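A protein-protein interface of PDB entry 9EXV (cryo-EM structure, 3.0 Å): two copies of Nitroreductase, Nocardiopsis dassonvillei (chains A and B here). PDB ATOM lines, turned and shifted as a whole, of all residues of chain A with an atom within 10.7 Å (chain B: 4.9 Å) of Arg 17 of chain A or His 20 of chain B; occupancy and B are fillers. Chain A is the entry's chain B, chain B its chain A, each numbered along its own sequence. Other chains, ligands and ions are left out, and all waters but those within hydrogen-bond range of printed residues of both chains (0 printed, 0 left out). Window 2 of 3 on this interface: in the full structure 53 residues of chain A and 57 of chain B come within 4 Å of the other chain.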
ATOM      1  N   PRO A  14     -10.635  10.589  14.226  1.00  0.00           N
ATOM      2  CA  PRO A  14     -11.891  10.272  13.539  1.00  0.00           C
ATOM      3  C   PRO A  14     -12.405   8.867  13.884  1.00  0.00           C
ATOM      4  O   PRO A  14     -13.026   8.710  14.934  1.00  0.00           O
ATOM      5  CB  PRO A  14     -11.519  10.399  12.054  1.00  0.00           C
ATOM      6  CG  PRO A  14     -10.032  10.257  12.010  1.00  0.00           C
ATOM      7  CD  PRO A  14      -9.545  10.880  13.280  1.00  0.00           C
ATOM      8  N   SER A  15     -12.163   7.874  13.026  1.00  0.00           N
ATOM      9  CA  SER A  15     -12.643   6.524  13.318  1.00  0.00           C
ATOM     10  C   SER A  15     -11.868   5.896  14.467  1.00  0.00           C
ATOM     11  O   SER A  15     -12.447   5.208  15.315  1.00  0.00           O
ATOM     12  CB  SER A  15     -12.555   5.651  12.067  1.00  0.00           C
ATOM     13  OG  SER A  15     -11.204   5.449  11.686  1.00  0.00           O
ATOM     14  N   GLN A  16     -10.553   6.120  14.510  1.00  0.00           N
ATOM     15  CA  GLN A  16      -9.740   5.510  15.555  1.00  0.00           C
ATOM     16  C   GLN A  16      -9.994   6.165  16.907  1.00  0.00           C
ATOM     17  O   GLN A  16     -10.040   5.480  17.935  1.00  0.00           O
ATOM     18  CB  GLN A  16      -8.255   5.576  15.182  1.00  0.00           C
ATOM     19  CG  GLN A  16      -7.691   6.978  14.958  1.00  0.00           C
ATOM     20  CD  GLN A  16      -7.805   7.447  13.517  1.00  0.00           C
ATOM     21  OE1 GLN A  16      -8.470   6.817  12.694  1.00  0.00           O
ATOM     22  NE2 GLN A  16      -7.143   8.554  13.204  1.00  0.00           N
ATOM     23  N   ARG A  17     -10.168   7.488  16.924  1.00  0.00           N
ATOM     24  CA  ARG A  17     -10.489   8.169  18.173  1.00  0.00           C
ATOM     25  C   ARG A  17     -11.842   7.717  18.707  1.00  0.00           C
ATOM     26  O   ARG A  17     -11.992   7.467  19.910  1.00  0.00           O
ATOM     27  CB  ARG A  17     -10.469   9.681  17.961  1.00  0.00           C
ATOM     28  CG  ARG A  17     -10.448  10.496  19.241  1.00  0.00           C
ATOM     29  CD  ARG A  17     -10.517  11.983  18.944  1.00  0.00           C
ATOM     30  NE  ARG A  17     -11.871  12.401  18.603  1.00  0.00           N
ATOM     31  CZ  ARG A  17     -12.798  12.728  19.495  1.00  0.00           C
ATOM     32  NH1 ARG A  17     -12.545  12.709  20.790  1.00  0.00           N
ATOM     33  NH2 ARG A  17     -14.009  13.079  19.072  1.00  0.00           N
ATOM     34  N   SER A  18     -12.837   7.601  17.826  1.00  0.00           N
ATOM     35  CA  SER A  18     -14.144   7.112  18.248  1.00  0.00           C
ATOM     36  C   SER A  18     -14.058   5.683  18.763  1.00  0.00           C
ATOM     37  O   SER A  18     -14.664   5.346  19.786  1.00  0.00           O
ATOM     38  CB  SER A  18     -15.142   7.205  17.095  1.00  0.00           C
ATOM     39  OG  SER A  18     -14.784   6.330  16.040  1.00  0.00           O
ATOM     40  N   SER A  19     -13.306   4.827  18.069  1.00  0.00           N
ATOM     41  CA  SER A  19     -13.164   3.446  18.517  1.00  0.00           C
ATOM     42  C   SER A  19     -12.494   3.377  19.884  1.00  0.00           C
ATOM     43  O   SER A  19     -12.922   2.611  20.756  1.00  0.00           O
ATOM     44  CB  SER A  19     -12.373   2.640  17.488  1.00  0.00           C
ATOM     45  OG  SER A  19     -13.069   2.568  16.256  1.00  0.00           O
ATOM     46  N   HIS A  20     -11.444   4.175  20.090  1.00  0.00           N
ATOM     47  CA  HIS A  20     -10.772   4.196  21.384  1.00  0.00           C
ATOM     48  C   HIS A  20     -11.704   4.688  22.482  1.00  0.00           C
ATOM     49  O   HIS A  20     -11.729   4.125  23.584  1.00  0.00           O
ATOM     50  CB  HIS A  20      -9.520   5.068  21.312  1.00  0.00           C
ATOM     51  CG  HIS A  20      -8.406   4.461  20.520  1.00  0.00           C
ATOM     52  ND1 HIS A  20      -7.308   5.184  20.103  1.00  0.00           N
ATOM     53  CD2 HIS A  20      -8.217   3.198  20.071  1.00  0.00           C
ATOM     54  CE1 HIS A  20      -6.492   4.391  19.430  1.00  0.00           C
ATOM     55  NE2 HIS A  20      -7.020   3.181  19.397  1.00  0.00           N
ATOM     56  N   ALA A  21     -12.476   5.739  22.205  1.00  0.00           N
ATOM     57  CA  ALA A  21     -13.416   6.236  23.203  1.00  0.00           C
ATOM     58  C   ALA A  21     -14.466   5.189  23.541  1.00  0.00           C
ATOM     59  O   ALA A  21     -14.781   4.974  24.709  1.00  0.00           O
ATOM     60  CB  ALA A  21     -14.074   7.519  22.709  1.00  0.00           C
ATOM     61  N   LEU A  22     -15.004   4.511  22.528  1.00  0.00           N
ATOM     62  CA  LEU A  22     -16.012   3.487  22.783  1.00  0.00           C
ATOM     63  C   LEU A  22     -15.428   2.331  23.583  1.00  0.00           C
ATOM     64  O   LEU A  22     -16.091   1.783  24.470  1.00  0.00           O
ATOM     65  CB  LEU A  22     -16.610   2.992  21.469  1.00  0.00           C
ATOM     66  CG  LEU A  22     -17.848   3.751  20.984  1.00  0.00           C
ATOM     67  CD1 LEU A  22     -19.033   3.490  21.896  1.00  0.00           C
ATOM     68  CD2 LEU A  22     -17.576   5.234  20.892  1.00  0.00           C
ATOM     69  N   GLN A  23     -14.187   1.946  23.283  1.00  0.00           N
ATOM     70  CA  GLN A  23     -13.523   0.933  24.094  1.00  0.00           C
ATOM     71  C   GLN A  23     -13.390   1.395  25.538  1.00  0.00           C
ATOM     72  O   GLN A  23     -13.653   0.628  26.468  1.00  0.00           O
ATOM     73  CB  GLN A  23     -12.149   0.607  23.511  1.00  0.00           C
ATOM     74  CG  GLN A  23     -11.512  -0.646  24.091  1.00  0.00           C
ATOM     75  CD  GLN A  23     -12.240  -1.916  23.683  1.00  0.00           C
ATOM     76  OE1 GLN A  23     -12.466  -2.805  24.504  1.00  0.00           O
ATOM     77  NE2 GLN A  23     -12.599  -2.011  22.408  1.00  0.00           N
ATOM     78  N   THR A  24     -13.001   2.656  25.738  1.00  0.00           N
ATOM     79  CA  THR A  24     -12.860   3.189  27.088  1.00  0.00           C
ATOM     80  C   THR A  24     -14.183   3.139  27.840  1.00  0.00           C
ATOM     81  O   THR A  24     -14.230   2.740  29.009  1.00  0.00           O
ATOM     82  CB  THR A  24     -12.332   4.625  27.019  1.00  0.00           C
ATOM     83  OG1 THR A  24     -11.076   4.640  26.331  1.00  0.00           O
ATOM     84  CG2 THR A  24     -12.149   5.220  28.412  1.00  0.00           C
ATOM     85  N   LEU A  25     -15.273   3.536  27.180  1.00  0.00           N
ATOM     86  CA  LEU A  25     -16.578   3.539  27.833  1.00  0.00           C
ATOM     87  C   LEU A  25     -17.057   2.125  28.135  1.00  0.00           C
ATOM     88  O   LEU A  25     -17.613   1.869  29.210  1.00  0.00           O
ATOM     89  CB  LEU A  25     -17.598   4.275  26.965  1.00  0.00           C
ATOM     90  CG  LEU A  25     -17.612   5.803  27.055  1.00  0.00           C
ATOM     91  CD1 LEU A  25     -16.385   6.437  26.445  1.00  0.00           C
ATOM     92  CD2 LEU A  25     -18.853   6.344  26.391  1.00  0.00           C
ATOM     93  N   PRO A  46      -7.888  16.319  36.549  1.00  0.00           N
ATOM     94  CA  PRO A  46      -8.648  15.956  35.343  1.00  0.00           C
ATOM     95  C   PRO A  46      -9.929  15.206  35.651  1.00  0.00           C
ATOM     96  O   PRO A  46     -10.945  15.408  34.975  1.00  0.00           O
ATOM     97  CB  PRO A  46      -7.654  15.094  34.548  1.00  0.00           C
ATOM     98  CG  PRO A  46      -6.602  14.690  35.533  1.00  0.00           C
ATOM     99  CD  PRO A  46      -6.508  15.803  36.503  1.00  0.00           C
ATOM    100  N   ALA A  50     -13.607  16.484  34.451  1.00  0.00           N
ATOM    101  CA  ALA A  50     -14.515  15.644  33.679  1.00  0.00           C
ATOM    102  C   ALA A  50     -15.833  15.438  34.414  1.00  0.00           C
ATOM    103  O   ALA A  50     -16.904  15.441  33.796  1.00  0.00           O
ATOM    104  CB  ALA A  50     -13.856  14.302  33.364  1.00  0.00           C
ATOM    105  N   LEU A 131     -16.142   7.201  34.463  1.00  0.00           N
ATOM    106  CA  LEU A 131     -15.463   7.103  33.182  1.00  0.00           C
ATOM    107  C   LEU A 131     -14.147   7.870  33.192  1.00  0.00           C
ATOM    108  O   LEU A 131     -13.186   7.452  32.539  1.00  0.00           O
ATOM    109  CB  LEU A 131     -16.387   7.582  32.064  1.00  0.00           C
ATOM    110  CG  LEU A 131     -17.652   6.736  31.886  1.00  0.00           C
ATOM    111  CD1 LEU A 131     -18.602   7.387  30.914  1.00  0.00           C
ATOM    112  CD2 LEU A 131     -17.314   5.326  31.420  1.00  0.00           C
ATOM    113  N   ALA A 132     -14.072   8.979  33.935  1.00  0.00           N
ATOM    114  CA  ALA A 132     -12.801   9.687  34.080  1.00  0.00           C
ATOM    115  C   ALA A 132     -11.772   8.838  34.815  1.00  0.00           C
ATOM    116  O   ALA A 132     -10.599   8.795  34.430  1.00  0.00           O
ATOM    117  CB  ALA A 132     -13.023  11.007  34.814  1.00  0.00           C
ATOM    118  N   HIS A 134     -11.586   5.681  34.719  1.00  0.00           N
ATOM    119  CA  HIS A 134     -11.054   4.769  33.720  1.00  0.00           C
ATOM    120  C   HIS A 134     -10.177   5.493  32.708  1.00  0.00           C
ATOM    121  O   HIS A 134      -9.270   4.881  32.130  1.00  0.00           O
ATOM    122  CB  HIS A 134     -12.175   4.020  33.002  1.00  0.00           C
ATOM    123  CG  HIS A 134     -11.768   2.656  32.540  1.00  0.00           C
ATOM    124  ND1 HIS A 134     -10.716   2.446  31.674  1.00  0.00           N
ATOM    125  CD2 HIS A 134     -12.255   1.429  32.843  1.00  0.00           C
ATOM    126  CE1 HIS A 134     -10.580   1.150  31.455  1.00  0.00           C
ATOM    127  NE2 HIS A 134     -11.502   0.511  32.152  1.00  0.00           N
ATOM    128  N   CYS A 135     -10.423   6.786  32.478  1.00  0.00           N
ATOM    129  CA  CYS A 135      -9.548   7.555  31.600  1.00  0.00           C
ATOM    130  C   CYS A 135      -8.124   7.579  32.137  1.00  0.00           C
ATOM    131  O   CYS A 135      -7.161   7.501  31.368  1.00  0.00           O
ATOM    132  CB  CYS A 135     -10.069   8.984  31.433  1.00  0.00           C
ATOM    133  SG  CYS A 135     -11.582   9.148  30.470  1.00  0.00           S
ATOM    134  N   LEU A 136      -7.969   7.686  33.453  1.00  0.00           N
ATOM    135  CA  LEU A 136      -6.656   7.738  34.075  1.00  0.00           C
ATOM    136  C   LEU A 136      -6.205   6.396  34.637  1.00  0.00           C
ATOM    137  O   LEU A 136      -5.207   6.343  35.360  1.00  0.00           O
ATOM    138  CB  LEU A 136      -6.632   8.803  35.169  1.00  0.00           C
ATOM    139  CG  LEU A 136      -6.821  10.223  34.636  1.00  0.00           C
ATOM    140  CD1 LEU A 136      -6.957  11.204  35.769  1.00  0.00           C
ATOM    141  CD2 LEU A 136      -5.663  10.614  33.728  1.00  0.00           C
ATOM    142  N   GLN B  16      -1.489   9.970  25.954  1.00  0.00           N
ATOM    143  CA  GLN B  16      -2.269  10.418  24.806  1.00  0.00           C
ATOM    144  C   GLN B  16      -3.701   9.901  24.865  1.00  0.00           C
ATOM    145  O   GLN B  16      -4.645  10.645  24.576  1.00  0.00           O
ATOM    146  CB  GLN B  16      -1.589  10.002  23.495  1.00  0.00           C
ATOM    147  CG  GLN B  16      -1.614   8.506  23.157  1.00  0.00           C
ATOM    148  CD  GLN B  16      -0.470   7.726  23.779  1.00  0.00           C
ATOM    149  OE1 GLN B  16       0.334   8.269  24.536  1.00  0.00           O
ATOM    150  NE2 GLN B  16      -0.387   6.441  23.451  1.00  0.00           N
ATOM    151  N   ARG B  17      -3.888   8.633  25.238  1.00  0.00           N
ATOM    152  CA  ARG B  17      -5.238   8.087  25.308  1.00  0.00           C
ATOM    153  C   ARG B  17      -5.997   8.652  26.498  1.00  0.00           C
ATOM    154  O   ARG B  17      -7.203   8.905  26.409  1.00  0.00           O
ATOM    155  CB  ARG B  17      -5.195   6.564  25.372  1.00  0.00           C
ATOM    156  CG  ARG B  17      -4.429   6.018  26.561  1.00  0.00           C
ATOM    157  CD  ARG B  17      -4.545   4.510  26.642  1.00  0.00           C
ATOM    158  NE  ARG B  17      -5.889   4.095  27.023  1.00  0.00           N
ATOM    159  CZ  ARG B  17      -6.330   4.045  28.273  1.00  0.00           C
ATOM    160  NH1 ARG B  17      -5.554   4.372  29.294  1.00  0.00           N
ATOM    161  NH2 ARG B  17      -7.582   3.659  28.504  1.00  0.00           N
ATOM    162  N   SER B  18      -5.309   8.851  27.625  1.00  0.00           N
ATOM    163  CA  SER B  18      -5.941   9.527  28.749  1.00  0.00           C
ATOM    164  C   SER B  18      -6.372  10.930  28.352  1.00  0.00           C
ATOM    165  O   SER B  18      -7.490  11.353  28.655  1.00  0.00           O
ATOM    166  CB  SER B  18      -4.989   9.571  29.943  1.00  0.00           C
ATOM    167  OG  SER B  18      -3.832  10.331  29.644  1.00  0.00           O
ATOM    168  N   SER B  19      -5.506  11.652  27.638  1.00  0.00           N
ATOM    169  CA  SER B  19      -5.860  12.987  27.172  1.00  0.00           C
ATOM    170  C   SER B  19      -7.049  12.947  26.218  1.00  0.00           C
ATOM    171  O   SER B  19      -7.965  13.769  26.327  1.00  0.00           O
ATOM    172  CB  SER B  19      -4.655  13.643  26.502  1.00  0.00           C
ATOM    173  OG  SER B  19      -5.033  14.805  25.786  1.00  0.00           O
ATOM    174  N   HIS B  20      -7.054  11.994  25.282  1.00  0.00           N
ATOM    175  CA  HIS B  20      -8.144  11.914  24.313  1.00  0.00           C
ATOM    176  C   HIS B  20      -9.470  11.576  24.981  1.00  0.00           C
ATOM    177  O   HIS B  20     -10.502  12.178  24.665  1.00  0.00           O
ATOM    178  CB  HIS B  20      -7.817  10.884  23.235  1.00  0.00           C
ATOM    179  CG  HIS B  20      -7.041  11.436  22.081  1.00  0.00           C
ATOM    180  ND1 HIS B  20      -7.530  11.438  20.792  1.00  0.00           N
ATOM    181  CD2 HIS B  20      -5.817  12.009  22.020  1.00  0.00           C
ATOM    182  CE1 HIS B  20      -6.638  11.985  19.986  1.00  0.00           C
ATOM    183  NE2 HIS B  20      -5.588  12.340  20.707  1.00  0.00           N
ATOM    184  N   ALA B  21      -9.465  10.600  25.889  1.00  0.00           N
ATOM    185  CA  ALA B  21     -10.694  10.242  26.588  1.00  0.00           C
ATOM    186  C   ALA B  21     -11.177  11.383  27.475  1.00  0.00           C
ATOM    187  O   ALA B  21     -12.381  11.642  27.564  1.00  0.00           O
ATOM    188  CB  ALA B  21     -10.477   8.968  27.396  1.00  0.00           C
ATOM    189  N   LEU B  22     -10.248  12.072  28.136  1.00  0.00           N
ATOM    190  CA  LEU B  22     -10.617  13.238  28.932  1.00  0.00           C
ATOM    191  C   LEU B  22     -11.216  14.332  28.057  1.00  0.00           C
ATOM    192  O   LEU B  22     -12.183  14.993  28.450  1.00  0.00           O
ATOM    193  CB  LEU B  22      -9.398  13.751  29.695  1.00  0.00           C
ATOM    194  CG  LEU B  22      -8.949  12.834  30.836  1.00  0.00           C
ATOM    195  CD1 LEU B  22      -7.532  13.157  31.287  1.00  0.00           C
ATOM    196  CD2 LEU B  22      -9.919  12.931  31.997  1.00  0.00           C
ATOM    197  N   GLN B  23     -10.648  14.539  26.868  1.00  0.00           N
ATOM    198  CA  GLN B  23     -11.197  15.529  25.947  1.00  0.00           C
ATOM    199  C   GLN B  23     -12.585  15.130  25.465  1.00  0.00           C
ATOM    200  O   GLN B  23     -13.474  15.977  25.352  1.00  0.00           O
ATOM    201  CB  GLN B  23     -10.249  15.723  24.765  1.00  0.00           C
ATOM    202  CG  GLN B  23      -8.942  16.406  25.131  1.00  0.00           C
ATOM    203  CD  GLN B  23      -9.147  17.813  25.649  1.00  0.00           C
ATOM    204  OE1 GLN B  23      -8.980  18.080  26.839  1.00  0.00           O
ATOM    205  NE2 GLN B  23      -9.510  18.724  24.755  1.00  0.00           N
ATOM    206  N   THR B  24     -12.787  13.844  25.170  1.00  0.00           N
ATOM    207  CA  THR B  24     -14.100  13.379  24.737  1.00  0.00           C
ATOM    208  C   THR B  24     -15.138  13.575  25.835  1.00  0.00           C
ATOM    209  O   THR B  24     -16.249  14.053  25.580  1.00  0.00           O
ATOM    210  CB  THR B  24     -14.024  11.907  24.328  1.00  0.00           C
ATOM    211  OG1 THR B  24     -13.056  11.745  23.287  1.00  0.00           O
ATOM    212  CG2 THR B  24     -15.379  11.412  23.839  1.00  0.00           C
ATOM    213  N   CYS B 135     -19.077  10.414  20.778  1.00  0.00           N
ATOM    214  CA  CYS B 135     -17.882   9.851  20.157  1.00  0.00           C
ATOM    215  C   CYS B 135     -18.072   9.649  18.659  1.00  0.00           C
ATOM    216  O   CYS B 135     -17.160   9.913  17.867  1.00  0.00           O
ATOM    217  CB  CYS B 135     -17.516   8.537  20.830  1.00  0.00           C
ATOM    218  SG  CYS B 135     -17.192   8.674  22.595  1.00  0.00           S
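The side-chain hydroxyl (OG1) of Thr 24 of chain B is in hydrogen-bond range of the guanidinium group (NH1) of Arg 17 of chain A.
The backbone carbonyl oxygen (O) of Leu 131 of chain A lies within hydrogen-bond range of the side-chain sulfur (SG) of Cys 135 of chain A.
The backbone carbonyl oxygen (O) of Pro 14 of chain A lies within hydrogen-bond range of the side-chain hydroxyl (OG) of Ser 18 of chain A (3.2 Å).
The backbone carbonyl oxygen (O) of His 20 of chain B sits at hydrogen-bond distance from the side-chain hydroxyl (OG1) of Thr 24 of chain B, at 2.9 Å.
OG of Ser 18 of chain A sits at hydrogen-bond distance from O of Ser 15 of chain A.
His 20 of chain B touches Arg 17 of chain A.
Cys 135 of chain B touches Ser 18 of chain A (O to CB, 3.5 Å).
Ala 21 of chain A touches Cys 135 of chain B.
Cys 135 of chain B touches Leu 22 of chain A.
Leu 22 of chain B touches Pro 46 of chain A (CD1 to CB, 3.8 Å).
Ser 18 of chain B touches Cys 135 of chain A.
Cys 135 of chain A touches Ala 21 of chain B.
N of Leu 22 of chain B touches SG of Cys 135 of chain A, at 3.97 Å.
Leu 136 of chain A touches Ser 18 of chain B.
Leu 136 of chain A touches Leu 22 of chain B (CD2 to CD1, 3.99 Å).
Arg 17 of chain A touches just these residues of chain B: His 20 (3.4 Å) and Thr 24 (2.7 Å).
His 20 of chain B touches one residue of chain A.
Ala 21 of chain B touches just one residue of chain A: Cys 135.
Cys 135 of chain B touches just these residues of chain A: Ser 18 (3.5 Å), Ala 21 (3.3 Å) and Leu 22 (3.3 Å).
Of the printed residues of chain B, Pro 46 of chain A touches Leu 22.
Of the printed residues of chain A, Ser 18 of chain B touches Cys 135 and Leu 136.
Of the printed residues of chain B, Cys 135 of chain A touches Ser 18 (3.3 Å), Ala 21 (3.3 Å) and Leu 22 (3.97 Å).
Printed residues of chain B within 4 Å of Ser 18 of chain A: Cys 135.
Printed residues of chain B within 4 Å of Ala 21 of chain A: Cys 135.
The nearest residue of chain B that does not touch Arg 17 of chain A is Cys 135 of chain B (4.6 Å).
The nearest residue of chain A that does not touch His 20 of chain B is Ala 21 of chain A (6.2 Å).
The nearest printed residue of chain B that does not touch Ser 18 of chain A is Thr 24 of chain B (6.9 Å).
Of the 19 printed residues of chain A, 7 touch a printed residue of chain B.
Hydrophobic or aromatic side chains of chain A that line the printed part of chain B: Ala 21, Leu 22, Pro 46 and Leu 136.
Arg 17 of chain A touches His 20 of chain B, but with the chains exchanged His 20 of chain A does not touch Arg 17 of chain B (5.8 Å).
Arg 17 of chain A touches Thr 24 of chain B, but with the chains exchanged Thr 24 of chain A does not touch Arg 17 of chain B (4.2 Å).
Ala 21 of chain A touches Cys 135 of chain B, and with the chains exchanged Cys 135 of chain A touches Ala 21 of chain B.
Leu 22 of chain A touches Cys 135 of chain B, and with the chains exchanged Cys 135 of chain A touches Leu 22 of chain B.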
